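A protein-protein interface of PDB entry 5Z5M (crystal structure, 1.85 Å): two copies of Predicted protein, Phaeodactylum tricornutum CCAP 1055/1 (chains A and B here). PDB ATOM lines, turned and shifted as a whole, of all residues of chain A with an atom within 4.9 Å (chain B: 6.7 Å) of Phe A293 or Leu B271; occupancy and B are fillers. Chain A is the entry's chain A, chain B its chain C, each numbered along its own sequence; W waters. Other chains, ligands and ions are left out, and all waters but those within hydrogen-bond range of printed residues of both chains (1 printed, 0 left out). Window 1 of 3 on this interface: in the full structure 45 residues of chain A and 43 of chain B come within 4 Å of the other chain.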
ATOM      1  N   LEU A 266     -14.903  -9.634   4.871  1.00  0.00           N
ATOM      2  CA  LEU A 266     -14.391  -8.272   4.745  1.00  0.00           C
ATOM      3  C   LEU A 266     -14.128  -7.954   3.284  1.00  0.00           C
ATOM      4  O   LEU A 266     -13.434  -8.708   2.611  1.00  0.00           O
ATOM      5  CB  LEU A 266     -13.089  -8.097   5.527  1.00  0.00           C
ATOM      6  CG  LEU A 266     -13.103  -8.188   7.050  1.00  0.00           C
ATOM      7  CD1 LEU A 266     -11.684  -7.932   7.576  1.00  0.00           C
ATOM      8  CD2 LEU A 266     -14.098  -7.204   7.648  1.00  0.00           C
ATOM      9  N   ILE A 269     -13.780  -1.655   3.887  1.00  0.00           N
ATOM     10  CA  ILE A 269     -13.652  -1.361   5.315  1.00  0.00           C
ATOM     11  C   ILE A 269     -13.650   0.136   5.596  1.00  0.00           C
ATOM     12  O   ILE A 269     -12.747   0.855   5.148  1.00  0.00           O
ATOM     13  CB  ILE A 269     -12.361  -1.963   5.910  1.00  0.00           C
ATOM     14  CG1 ILE A 269     -12.346  -3.483   5.749  1.00  0.00           C
ATOM     15  CG2 ILE A 269     -12.198  -1.559   7.387  1.00  0.00           C
ATOM     16  CD1 ILE A 269     -11.106  -4.138   6.341  1.00  0.00           C
ATOM     17  N   LEU A 271     -13.063   3.209   8.202  1.00  0.00           N
ATOM     18  CA  LEU A 271     -12.276   3.474   9.404  1.00  0.00           C
ATOM     19  C   LEU A 271     -12.514   4.911   9.825  1.00  0.00           C
ATOM     20  O   LEU A 271     -11.931   5.836   9.258  1.00  0.00           O
ATOM     21  CB  LEU A 271     -10.782   3.223   9.158  1.00  0.00           C
ATOM     22  CG  LEU A 271      -9.961   2.622  10.305  1.00  0.00           C
ATOM     23  CD1 LEU A 271     -10.509   1.257  10.665  1.00  0.00           C
ATOM     24  CD2 LEU A 271      -8.476   2.516   9.938  1.00  0.00           C
ATOM     25  N   LEU A 286      -3.824   0.416   8.632  1.00  0.00           N
ATOM     26  CA  LEU A 286      -4.725  -0.726   8.656  1.00  0.00           C
ATOM     27  C   LEU A 286      -3.919  -2.030   8.662  1.00  0.00           C
ATOM     28  O   LEU A 286      -3.074  -2.252   7.790  1.00  0.00           O
ATOM     29  CB  LEU A 286      -5.671  -0.692   7.444  1.00  0.00           C
ATOM     30  CG  LEU A 286      -6.652  -1.859   7.305  1.00  0.00           C
ATOM     31  CD1 LEU A 286      -7.709  -1.791   8.405  1.00  0.00           C
ATOM     32  CD2 LEU A 286      -7.298  -1.882   5.924  1.00  0.00           C
ATOM     33  N   LEU A 287      -4.175  -2.881   9.652  1.00  0.00           N
ATOM     34  CA  LEU A 287      -3.661  -4.248   9.665  1.00  0.00           C
ATOM     35  C   LEU A 287      -4.802  -5.147   9.228  1.00  0.00           C
ATOM     36  O   LEU A 287      -5.848  -5.129   9.856  1.00  0.00           O
ATOM     37  CB  LEU A 287      -3.164  -4.648  11.059  1.00  0.00           C
ATOM     38  CG  LEU A 287      -1.809  -4.153  11.579  1.00  0.00           C
ATOM     39  CD1 LEU A 287      -1.727  -2.636  11.630  1.00  0.00           C
ATOM     40  CD2 LEU A 287      -1.538  -4.748  12.957  1.00  0.00           C
ATOM     41  N   VAL A 288      -4.637  -5.920   8.156  1.00  0.00           N
ATOM     42  CA  VAL A 288      -5.804  -6.626   7.626  1.00  0.00           C
ATOM     43  C   VAL A 288      -5.516  -8.015   7.035  1.00  0.00           C
ATOM     44  O   VAL A 288      -4.468  -8.249   6.437  1.00  0.00           O
ATOM     45  CB  VAL A 288      -6.507  -5.752   6.555  1.00  0.00           C
ATOM     46  CG1 VAL A 288      -5.576  -5.473   5.367  1.00  0.00           C
ATOM     47  CG2 VAL A 288      -7.805  -6.386   6.089  1.00  0.00           C
ATOM     48  N   TRP A 291     -10.077 -12.007   7.253  1.00  0.00           N
ATOM     49  CA  TRP A 291     -10.889 -12.457   8.383  1.00  0.00           C
ATOM     50  C   TRP A 291     -10.677 -11.629   9.642  1.00  0.00           C
ATOM     51  O   TRP A 291     -11.203 -11.960  10.704  1.00  0.00           O
ATOM     52  CB  TRP A 291     -10.588 -13.925   8.687  1.00  0.00           C
ATOM     53  CG  TRP A 291     -10.521 -14.774   7.453  1.00  0.00           C
ATOM     54  CD1 TRP A 291      -9.392 -15.183   6.803  1.00  0.00           C
ATOM     55  CD2 TRP A 291     -11.628 -15.309   6.710  1.00  0.00           C
ATOM     56  NE1 TRP A 291      -9.726 -15.941   5.708  1.00  0.00           N
ATOM     57  CE2 TRP A 291     -11.093 -16.034   5.629  1.00  0.00           C
ATOM     58  CE3 TRP A 291     -13.017 -15.248   6.857  1.00  0.00           C
ATOM     59  CZ2 TRP A 291     -11.896 -16.691   4.698  1.00  0.00           C
ATOM     60  CZ3 TRP A 291     -13.817 -15.907   5.929  1.00  0.00           C
ATOM     61  CH2 TRP A 291     -13.253 -16.613   4.865  1.00  0.00           C
ATOM     62  N   SER A 292      -9.916 -10.549   9.525  1.00  0.00           N
ATOM     63  CA  SER A 292      -9.600  -9.735  10.696  1.00  0.00           C
ATOM     64  C   SER A 292      -9.052  -8.386  10.293  1.00  0.00           C
ATOM     65  O   SER A 292      -8.469  -8.242   9.218  1.00  0.00           O
ATOM     66  CB  SER A 292      -8.584 -10.459  11.581  1.00  0.00           C
ATOM     67  OG  SER A 292      -7.317 -10.495  10.939  1.00  0.00           O
ATOM     68  N   PHE A 293      -9.224  -7.384  11.147  1.00  0.00           N
ATOM     69  CA  PHE A 293      -8.499  -6.154  10.930  1.00  0.00           C
ATOM     70  C   PHE A 293      -8.353  -5.368  12.222  1.00  0.00           C
ATOM     71  O   PHE A 293      -9.079  -5.591  13.199  1.00  0.00           O
ATOM     72  CB  PHE A 293      -9.152  -5.301   9.823  1.00  0.00           C
ATOM     73  CG  PHE A 293     -10.436  -4.619  10.214  1.00  0.00           C
ATOM     74  CD1 PHE A 293     -10.426  -3.320  10.696  1.00  0.00           C
ATOM     75  CD2 PHE A 293     -11.655  -5.242  10.022  1.00  0.00           C
ATOM     76  CE1 PHE A 293     -11.604  -2.675  11.030  1.00  0.00           C
ATOM     77  CE2 PHE A 293     -12.841  -4.599  10.345  1.00  0.00           C
ATOM     78  CZ  PHE A 293     -12.815  -3.320  10.858  1.00  0.00           C
ATOM     79  N   SER A 294      -7.380  -4.467  12.222  1.00  0.00           N
ATOM     80  CA  SER A 294      -7.124  -3.638  13.389  1.00  0.00           C
ATOM     81  C   SER A 294      -6.475  -2.325  12.981  1.00  0.00           C
ATOM     82  O   SER A 294      -5.929  -2.186  11.884  1.00  0.00           O
ATOM     83  CB  SER A 294      -6.234  -4.373  14.394  1.00  0.00           C
ATOM     84  OG  SER A 294      -4.988  -4.717  13.820  1.00  0.00           O
ATOM     85  N   THR A 295      -6.536  -1.356  13.879  1.00  0.00           N
ATOM     86  CA  THR A 295      -5.914  -0.073  13.649  1.00  0.00           C
ATOM     87  C   THR A 295      -5.557   0.527  14.997  1.00  0.00           C
ATOM     88  O   THR A 295      -5.952   0.007  16.048  1.00  0.00           O
ATOM     89  CB  THR A 295      -6.834   0.884  12.879  1.00  0.00           C
ATOM     90  OG1 THR A 295      -6.148   2.113  12.627  1.00  0.00           O
ATOM     91  CG2 THR A 295      -8.078   1.182  13.696  1.00  0.00           C
ATOM     92  N   LEU B 203     -27.239  -2.222  14.493  1.00  0.00           N
ATOM     93  CA  LEU B 203     -26.931  -3.082  13.362  1.00  0.00           C
ATOM     94  C   LEU B 203     -27.841  -2.727  12.188  1.00  0.00           C
ATOM     95  O   LEU B 203     -29.064  -2.639  12.338  1.00  0.00           O
ATOM     96  CB  LEU B 203     -27.090  -4.560  13.748  1.00  0.00           C
ATOM     97  CG  LEU B 203     -26.734  -5.632  12.707  1.00  0.00           C
ATOM     98  CD1 LEU B 203     -25.293  -5.505  12.246  1.00  0.00           C
ATOM     99  CD2 LEU B 203     -26.992  -7.006  13.274  1.00  0.00           C
ATOM    100  N   TYR B 243     -23.653  -6.402   6.175  1.00  0.00           N
ATOM    101  CA  TYR B 243     -24.174  -5.749   7.369  1.00  0.00           C
ATOM    102  C   TYR B 243     -23.185  -4.725   7.898  1.00  0.00           C
ATOM    103  O   TYR B 243     -22.048  -4.664   7.452  1.00  0.00           O
ATOM    104  CB  TYR B 243     -24.474  -6.780   8.455  1.00  0.00           C
ATOM    105  CG  TYR B 243     -25.552  -7.769   8.079  1.00  0.00           C
ATOM    106  CD1 TYR B 243     -25.281  -8.828   7.221  1.00  0.00           C
ATOM    107  CD2 TYR B 243     -26.837  -7.650   8.589  1.00  0.00           C
ATOM    108  CE1 TYR B 243     -26.268  -9.731   6.873  1.00  0.00           C
ATOM    109  CE2 TYR B 243     -27.828  -8.559   8.247  1.00  0.00           C
ATOM    110  CZ  TYR B 243     -27.535  -9.590   7.393  1.00  0.00           C
ATOM    111  OH  TYR B 243     -28.513 -10.499   7.050  1.00  0.00           O
ATOM    112  N   GLU B 244     -23.627  -3.923   8.857  1.00  0.00           N
ATOM    113  CA  GLU B 244     -22.729  -2.981   9.503  1.00  0.00           C
ATOM    114  C   GLU B 244     -23.140  -2.745  10.942  1.00  0.00           C
ATOM    115  O   GLU B 244     -24.257  -2.294  11.207  1.00  0.00           O
ATOM    116  CB  GLU B 244     -22.695  -1.649   8.754  1.00  0.00           C
ATOM    117  CG  GLU B 244     -21.518  -0.760   9.146  1.00  0.00           C
ATOM    118  CD  GLU B 244     -21.457   0.519   8.321  1.00  0.00           C
ATOM    119  OE1 GLU B 244     -20.776   0.527   7.271  1.00  0.00           O
ATOM    120  OE2 GLU B 244     -22.095   1.515   8.723  1.00  0.00           O
ATOM    121  N   TRP B 245     -22.244  -3.080  11.863  1.00  0.00           N
ATOM    122  CA  TRP B 245     -22.399  -2.672  13.253  1.00  0.00           C
ATOM    123  C   TRP B 245     -22.083  -1.191  13.383  1.00  0.00           C
ATOM    124  O   TRP B 245     -21.215  -0.665  12.673  1.00  0.00           O
ATOM    125  CB  TRP B 245     -21.451  -3.411  14.193  1.00  0.00           C
ATOM    126  CG  TRP B 245     -21.541  -4.893  14.355  1.00  0.00           C
ATOM    127  CD1 TRP B 245     -20.608  -5.805  13.965  1.00  0.00           C
ATOM    128  CD2 TRP B 245     -22.558  -5.633  15.046  1.00  0.00           C
ATOM    129  NE1 TRP B 245     -20.991  -7.069  14.336  1.00  0.00           N
ATOM    130  CE2 TRP B 245     -22.188  -6.992  14.999  1.00  0.00           C
ATOM    131  CE3 TRP B 245     -23.755  -5.282  15.678  1.00  0.00           C
ATOM    132  CZ2 TRP B 245     -22.972  -7.999  15.558  1.00  0.00           C
ATOM    133  CZ3 TRP B 245     -24.530  -6.283  16.232  1.00  0.00           C
ATOM    134  CH2 TRP B 245     -24.134  -7.623  16.175  1.00  0.00           C
ATOM    135  N   THR B 246     -22.749  -0.534  14.322  1.00  0.00           N
ATOM    136  CA  THR B 246     -22.311   0.776  14.782  1.00  0.00           C
ATOM    137  C   THR B 246     -22.075   0.690  16.285  1.00  0.00           C
ATOM    138  O   THR B 246     -23.030   0.510  17.040  1.00  0.00           O
ATOM    139  CB  THR B 246     -23.353   1.867  14.459  1.00  0.00           C
ATOM    140  OG1 THR B 246     -23.566   1.921  13.046  1.00  0.00           O
ATOM    141  CG2 THR B 246     -22.878   3.219  14.942  1.00  0.00           C
ATOM    142  N   PHE B 247     -20.818   0.785  16.723  1.00  0.00           N
ATOM    143  CA  PHE B 247     -20.523   0.773  18.158  1.00  0.00           C
ATOM    144  C   PHE B 247     -20.358   2.186  18.692  1.00  0.00           C
ATOM    145  O   PHE B 247     -19.531   2.951  18.192  1.00  0.00           O
ATOM    146  CB  PHE B 247     -19.249  -0.022  18.470  1.00  0.00           C
ATOM    147  CG  PHE B 247     -19.311  -1.468  18.080  1.00  0.00           C
ATOM    148  CD1 PHE B 247     -19.762  -2.422  18.977  1.00  0.00           C
ATOM    149  CD2 PHE B 247     -18.891  -1.876  16.825  1.00  0.00           C
ATOM    150  CE1 PHE B 247     -19.814  -3.761  18.623  1.00  0.00           C
ATOM    151  CE2 PHE B 247     -18.933  -3.215  16.464  1.00  0.00           C
ATOM    152  CZ  PHE B 247     -19.399  -4.155  17.363  1.00  0.00           C
ATOM    153  N   ILE B 269     -17.803   3.687  16.067  1.00  0.00           N
ATOM    154  CA  ILE B 269     -17.047   2.760  15.234  1.00  0.00           C
ATOM    155  C   ILE B 269     -17.948   1.917  14.333  1.00  0.00           C
ATOM    156  O   ILE B 269     -18.721   1.084  14.819  1.00  0.00           O
ATOM    157  CB  ILE B 269     -16.179   1.813  16.097  1.00  0.00           C
ATOM    158  CG1 ILE B 269     -15.188   2.617  16.951  1.00  0.00           C
ATOM    159  CG2 ILE B 269     -15.448   0.806  15.222  1.00  0.00           C
ATOM    160  CD1 ILE B 269     -14.301   1.751  17.835  1.00  0.00           C
ATOM    161  N   PRO B 270     -17.847   2.128  13.010  1.00  0.00           N
ATOM    162  CA  PRO B 270     -18.566   1.267  12.065  1.00  0.00           C
ATOM    163  C   PRO B 270     -17.797  -0.019  11.808  1.00  0.00           C
ATOM    164  O   PRO B 270     -16.572   0.003  11.706  1.00  0.00           O
ATOM    165  CB  PRO B 270     -18.640   2.124  10.801  1.00  0.00           C
ATOM    166  CG  PRO B 270     -17.373   2.928  10.842  1.00  0.00           C
ATOM    167  CD  PRO B 270     -17.109   3.205  12.324  1.00  0.00           C
ATOM    168  N   LEU B 271     -18.505  -1.133  11.701  1.00  0.00           N
ATOM    169  CA  LEU B 271     -17.858  -2.403  11.416  1.00  0.00           C
ATOM    170  C   LEU B 271     -18.662  -3.116  10.345  1.00  0.00           C
ATOM    171  O   LEU B 271     -19.724  -3.663  10.616  1.00  0.00           O
ATOM    172  CB  LEU B 271     -17.726  -3.241  12.692  1.00  0.00           C
ATOM    173  CG  LEU B 271     -17.147  -4.659  12.639  1.00  0.00           C
ATOM    174  CD1 LEU B 271     -16.068  -4.792  11.591  1.00  0.00           C
ATOM    175  CD2 LEU B 271     -16.618  -5.055  14.018  1.00  0.00           C
ATOM    176  N   ARG B 272     -18.147  -3.086   9.120  1.00  0.00           N
ATOM    177  CA  ARG B 272     -18.874  -3.594   7.964  1.00  0.00           C
ATOM    178  C   ARG B 272     -18.402  -4.999   7.612  1.00  0.00           C
ATOM    179  O   ARG B 272     -17.202  -5.237   7.446  1.00  0.00           O
ATOM    180  CB  ARG B 272     -18.696  -2.640   6.784  1.00  0.00           C
ATOM    181  CG  ARG B 272     -19.577  -2.922   5.581  1.00  0.00           C
ATOM    182  CD  ARG B 272     -19.332  -1.891   4.491  1.00  0.00           C
ATOM    183  NE  ARG B 272     -19.610  -0.538   4.964  1.00  0.00           N
ATOM    184  CZ  ARG B 272     -19.210   0.568   4.344  1.00  0.00           C
ATOM    185  NH1 ARG B 272     -18.505   0.489   3.223  1.00  0.00           N
ATOM    186  NH2 ARG B 272     -19.507   1.755   4.849  1.00  0.00           N
ATOM    187  N   PHE B 273     -19.346  -5.935   7.506  1.00  0.00           N
ATOM    188  CA  PHE B 273     -18.994  -7.338   7.335  1.00  0.00           C
ATOM    189  C   PHE B 273     -20.050  -8.088   6.531  1.00  0.00           C
ATOM    190  O   PHE B 273     -21.203  -7.667   6.464  1.00  0.00           O
ATOM    191  CB  PHE B 273     -18.795  -8.014   8.697  1.00  0.00           C
ATOM    192  CG  PHE B 273     -20.063  -8.158   9.503  1.00  0.00           C
ATOM    193  CD1 PHE B 273     -20.529  -7.114  10.282  1.00  0.00           C
ATOM    194  CD2 PHE B 273     -20.780  -9.343   9.487  1.00  0.00           C
ATOM    195  CE1 PHE B 273     -21.691  -7.244  11.022  1.00  0.00           C
ATOM    196  CE2 PHE B 273     -21.943  -9.483  10.233  1.00  0.00           C
ATOM    197  CZ  PHE B 273     -22.401  -8.433  10.995  1.00  0.00           C
ATOM    198  N   VAL B 284     -18.908 -11.790  15.832  1.00  0.00           N
ATOM    199  CA  VAL B 284     -18.181 -10.655  15.272  1.00  0.00           C
ATOM    200  C   VAL B 284     -17.942  -9.618  16.361  1.00  0.00           C
ATOM    201  O   VAL B 284     -18.726  -8.683  16.517  1.00  0.00           O
ATOM    202  CB  VAL B 284     -18.950 -10.030  14.082  1.00  0.00           C
ATOM    203  CG1 VAL B 284     -18.156  -8.908  13.455  1.00  0.00           C
ATOM    204  CG2 VAL B 284     -19.258 -11.095  13.029  1.00  0.00           C
ATOM    205  N   PRO B 285     -16.861  -9.799  17.134  1.00  0.00           N
ATOM    206  CA  PRO B 285     -16.619  -8.996  18.332  1.00  0.00           C
ATOM    207  C   PRO B 285     -15.787  -7.742  18.088  1.00  0.00           C
ATOM    208  O   PRO B 285     -15.243  -7.520  17.003  1.00  0.00           O
ATOM    209  CB  PRO B 285     -15.857  -9.965  19.235  1.00  0.00           C
ATOM    210  CG  PRO B 285     -15.068 -10.788  18.279  1.00  0.00           C
ATOM    211  CD  PRO B 285     -15.879 -10.891  17.006  1.00  0.00           C
ATOM    212  N   LEU B 286     -15.687  -6.928  19.129  1.00  0.00           N
ATOM    213  CA  LEU B 286     -14.866  -5.734  19.085  1.00  0.00           C
ATOM    214  C   LEU B 286     -13.955  -5.690  20.301  1.00  0.00           C
ATOM    215  O   LEU B 286     -14.403  -5.843  21.436  1.00  0.00           O
ATOM    216  CB  LEU B 286     -15.735  -4.479  19.033  1.00  0.00           C
ATOM    217  CG  LEU B 286     -15.006  -3.135  19.006  1.00  0.00           C
ATOM    218  CD1 LEU B 286     -14.228  -2.978  17.706  1.00  0.00           C
ATOM    219  CD2 LEU B 286     -15.995  -1.990  19.195  1.00  0.00           C
ATOM    220  N   PHE B 293      -8.465  -0.373  17.935  1.00  0.00           N
ATOM    221  CA  PHE B 293      -9.464  -1.424  17.989  1.00  0.00           C
ATOM    222  C   PHE B 293      -9.148  -2.509  16.979  1.00  0.00           C
ATOM    223  O   PHE B 293      -8.377  -2.300  16.040  1.00  0.00           O
ATOM    224  CB  PHE B 293     -10.885  -0.863  17.783  1.00  0.00           C
ATOM    225  CG  PHE B 293     -11.207  -0.465  16.367  1.00  0.00           C
ATOM    226  CD1 PHE B 293     -11.749  -1.384  15.476  1.00  0.00           C
ATOM    227  CD2 PHE B 293     -11.017   0.839  15.939  1.00  0.00           C
ATOM    228  CE1 PHE B 293     -12.060  -1.018  14.186  1.00  0.00           C
ATOM    229  CE2 PHE B 293     -11.330   1.211  14.644  1.00  0.00           C
ATOM    230  CZ  PHE B 293     -11.847   0.281  13.767  1.00  0.00           C
ATOM    231  N   SER B 294      -9.732  -3.678  17.212  1.00  0.00           N
ATOM    232  CA  SER B 294      -9.542  -4.830  16.351  1.00  0.00           C
ATOM    233  C   SER B 294     -10.813  -5.650  16.320  1.00  0.00           C
ATOM    234  O   SER B 294     -11.629  -5.590  17.243  1.00  0.00           O
ATOM    235  CB  SER B 294      -8.378  -5.688  16.840  1.00  0.00           C
ATOM    236  OG  SER B 294      -8.476  -5.895  18.235  1.00  0.00           O
ATOM    237  N   THR B 295     -10.978  -6.417  15.253  1.00  0.00           N
ATOM    238  CA  THR B 295     -12.094  -7.335  15.165  1.00  0.00           C
ATOM    239  C   THR B 295     -11.701  -8.514  14.292  1.00  0.00           C
ATOM    240  O   THR B 295     -10.671  -8.484  13.606  1.00  0.00           O
ATOM    241  CB  THR B 295     -13.342  -6.662  14.593  1.00  0.00           C
ATOM    242  OG1 THR B 295     -14.458  -7.559  14.695  1.00  0.00           O
ATOM    243  CG2 THR B 295     -13.120  -6.321  13.137  1.00  0.00           C
ATOM    244  N   TYR B 296     -12.520  -9.554  14.315  1.00  0.00           N
ATOM    245  CA  TYR B 296     -12.209 -10.756  13.564  1.00  0.00           C
ATOM    246  C   TYR B 296     -13.446 -11.610  13.378  1.00  0.00           C
ATOM    247  O   TYR B 296     -14.466 -11.392  14.033  1.00  0.00           O
ATOM    248  CB  TYR B 296     -11.121 -11.565  14.273  1.00  0.00           C
ATOM    249  CG  TYR B 296     -11.453 -11.900  15.708  1.00  0.00           C
ATOM    250  CD1 TYR B 296     -12.248 -12.999  16.023  1.00  0.00           C
ATOM    251  CD2 TYR B 296     -10.971 -11.119  16.752  1.00  0.00           C
ATOM    252  CE1 TYR B 296     -12.552 -13.309  17.334  1.00  0.00           C
ATOM    253  CE2 TYR B 296     -11.273 -11.419  18.065  1.00  0.00           C
ATOM    254  CZ  TYR B 296     -12.062 -12.516  18.352  1.00  0.00           C
ATOM    255  OH  TYR B 296     -12.362 -12.818  19.662  1.00  0.00           O
HETATM  256  O   HOH W   1      -5.360  -2.730  17.242  1.00  0.00           O
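Of the 11 printed residues of chain A, 7 touch a printed residue of chain B. Hydrophobic or aromatic side chains of chain A that line the printed part of chain B: Leu A266, Leu A271 and Phe A293. Among the printed residues, 12 pairs touch across the chains. Among the printed residues, no Asp or Glu carboxylate lies within 4 Å of a Lys or Arg side-chain nitrogen of the other chain.
Leu A266 touches Arg B272. CZ of Phe B293 touches CD1 of Leu A271 (3.5 Å). Tyr B296 touches Trp A291 (CA to O, 3.3 Å). CA of Ser A292 touches O of Thr B295, 3.3 Å away. Tyr B296 touches Ser A292. Phe A293 touches Leu B271 (CE2 to CD1, 3.5 Å). Phe B293 touches Phe A293. Ser B294 touches Phe A293 (CA to O, 3.3 Å). Ser A294 touches Phe B293 (CA to O, 3.2 Å). CB of Ser A294 touches CB of Ser B294 (3.5 Å).
The backbone NH (N) of Ser A294 lies within hydrogen-bond range of the backbone carbonyl oxygen (O) of Leu A287 (2.9 Å). The backbone NH (N) of Trp B245 is in hydrogen-bond range of the backbone carbonyl oxygen (O) of Leu B271 (2.9 Å). NE of Arg B272 is in salt-bridge range of OE1 of Glu B244 (2.8 Å). O of Pro B285 lies within hydrogen-bond range of OG1 of Thr B295 (2.4 Å).
Water W1 lies within hydrogen-bond range of the backbone carbonyl oxygen (O) of Thr A295 (3.0 Å) and the backbone carbonyl oxygen (O) of Phe B293 (3.3 Å).
Leu A271 touches Phe B293, and with the chains exchanged Phe A293 touches Leu B271. Phe A293 touches Ser B294, and with the chains exchanged Ser A294 touches Phe B293. Phe A293 touches Thr B295, and with the chains exchanged Thr A295 touches Phe B293. Ser B294 touches its own counterpart, Ser A294.
N of Thr A295 lies within hydrogen-bond range of O of Phe B293 (3.0 Å). The backbone carbonyl oxygen (O) of Phe A293 is in hydrogen-bond range of the backbone NH (N) of Thr B295 (2.9 Å).
Of the printed residues of chain B, Trp A291 touches Tyr B296. Of the printed residues of chain B, Ser A292 touches Thr B295 and Tyr B296. Glu B244 touches none of the printed residues of chain A. Leu B271 touches one residue of chain A. Printed residues of chain A within 4 Å of Arg B272: Leu A266 (3.7 Å). Val B284 touches none of the printed residues of chain A. Of the printed residues of chain A, Phe B293 touches Leu A271 (3.5 Å), Phe A293 (3.6 Å), Ser A294 (3.2 Å) and Thr A295 (3.0 Å). Of the printed residues of chain A, Ser B294 touches Phe A293 (3.3 Å) and Ser A294 (3.5 Å). The nearest printed residue of chain A that does not touch Leu B271 is Leu A266 (5.0 Å).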
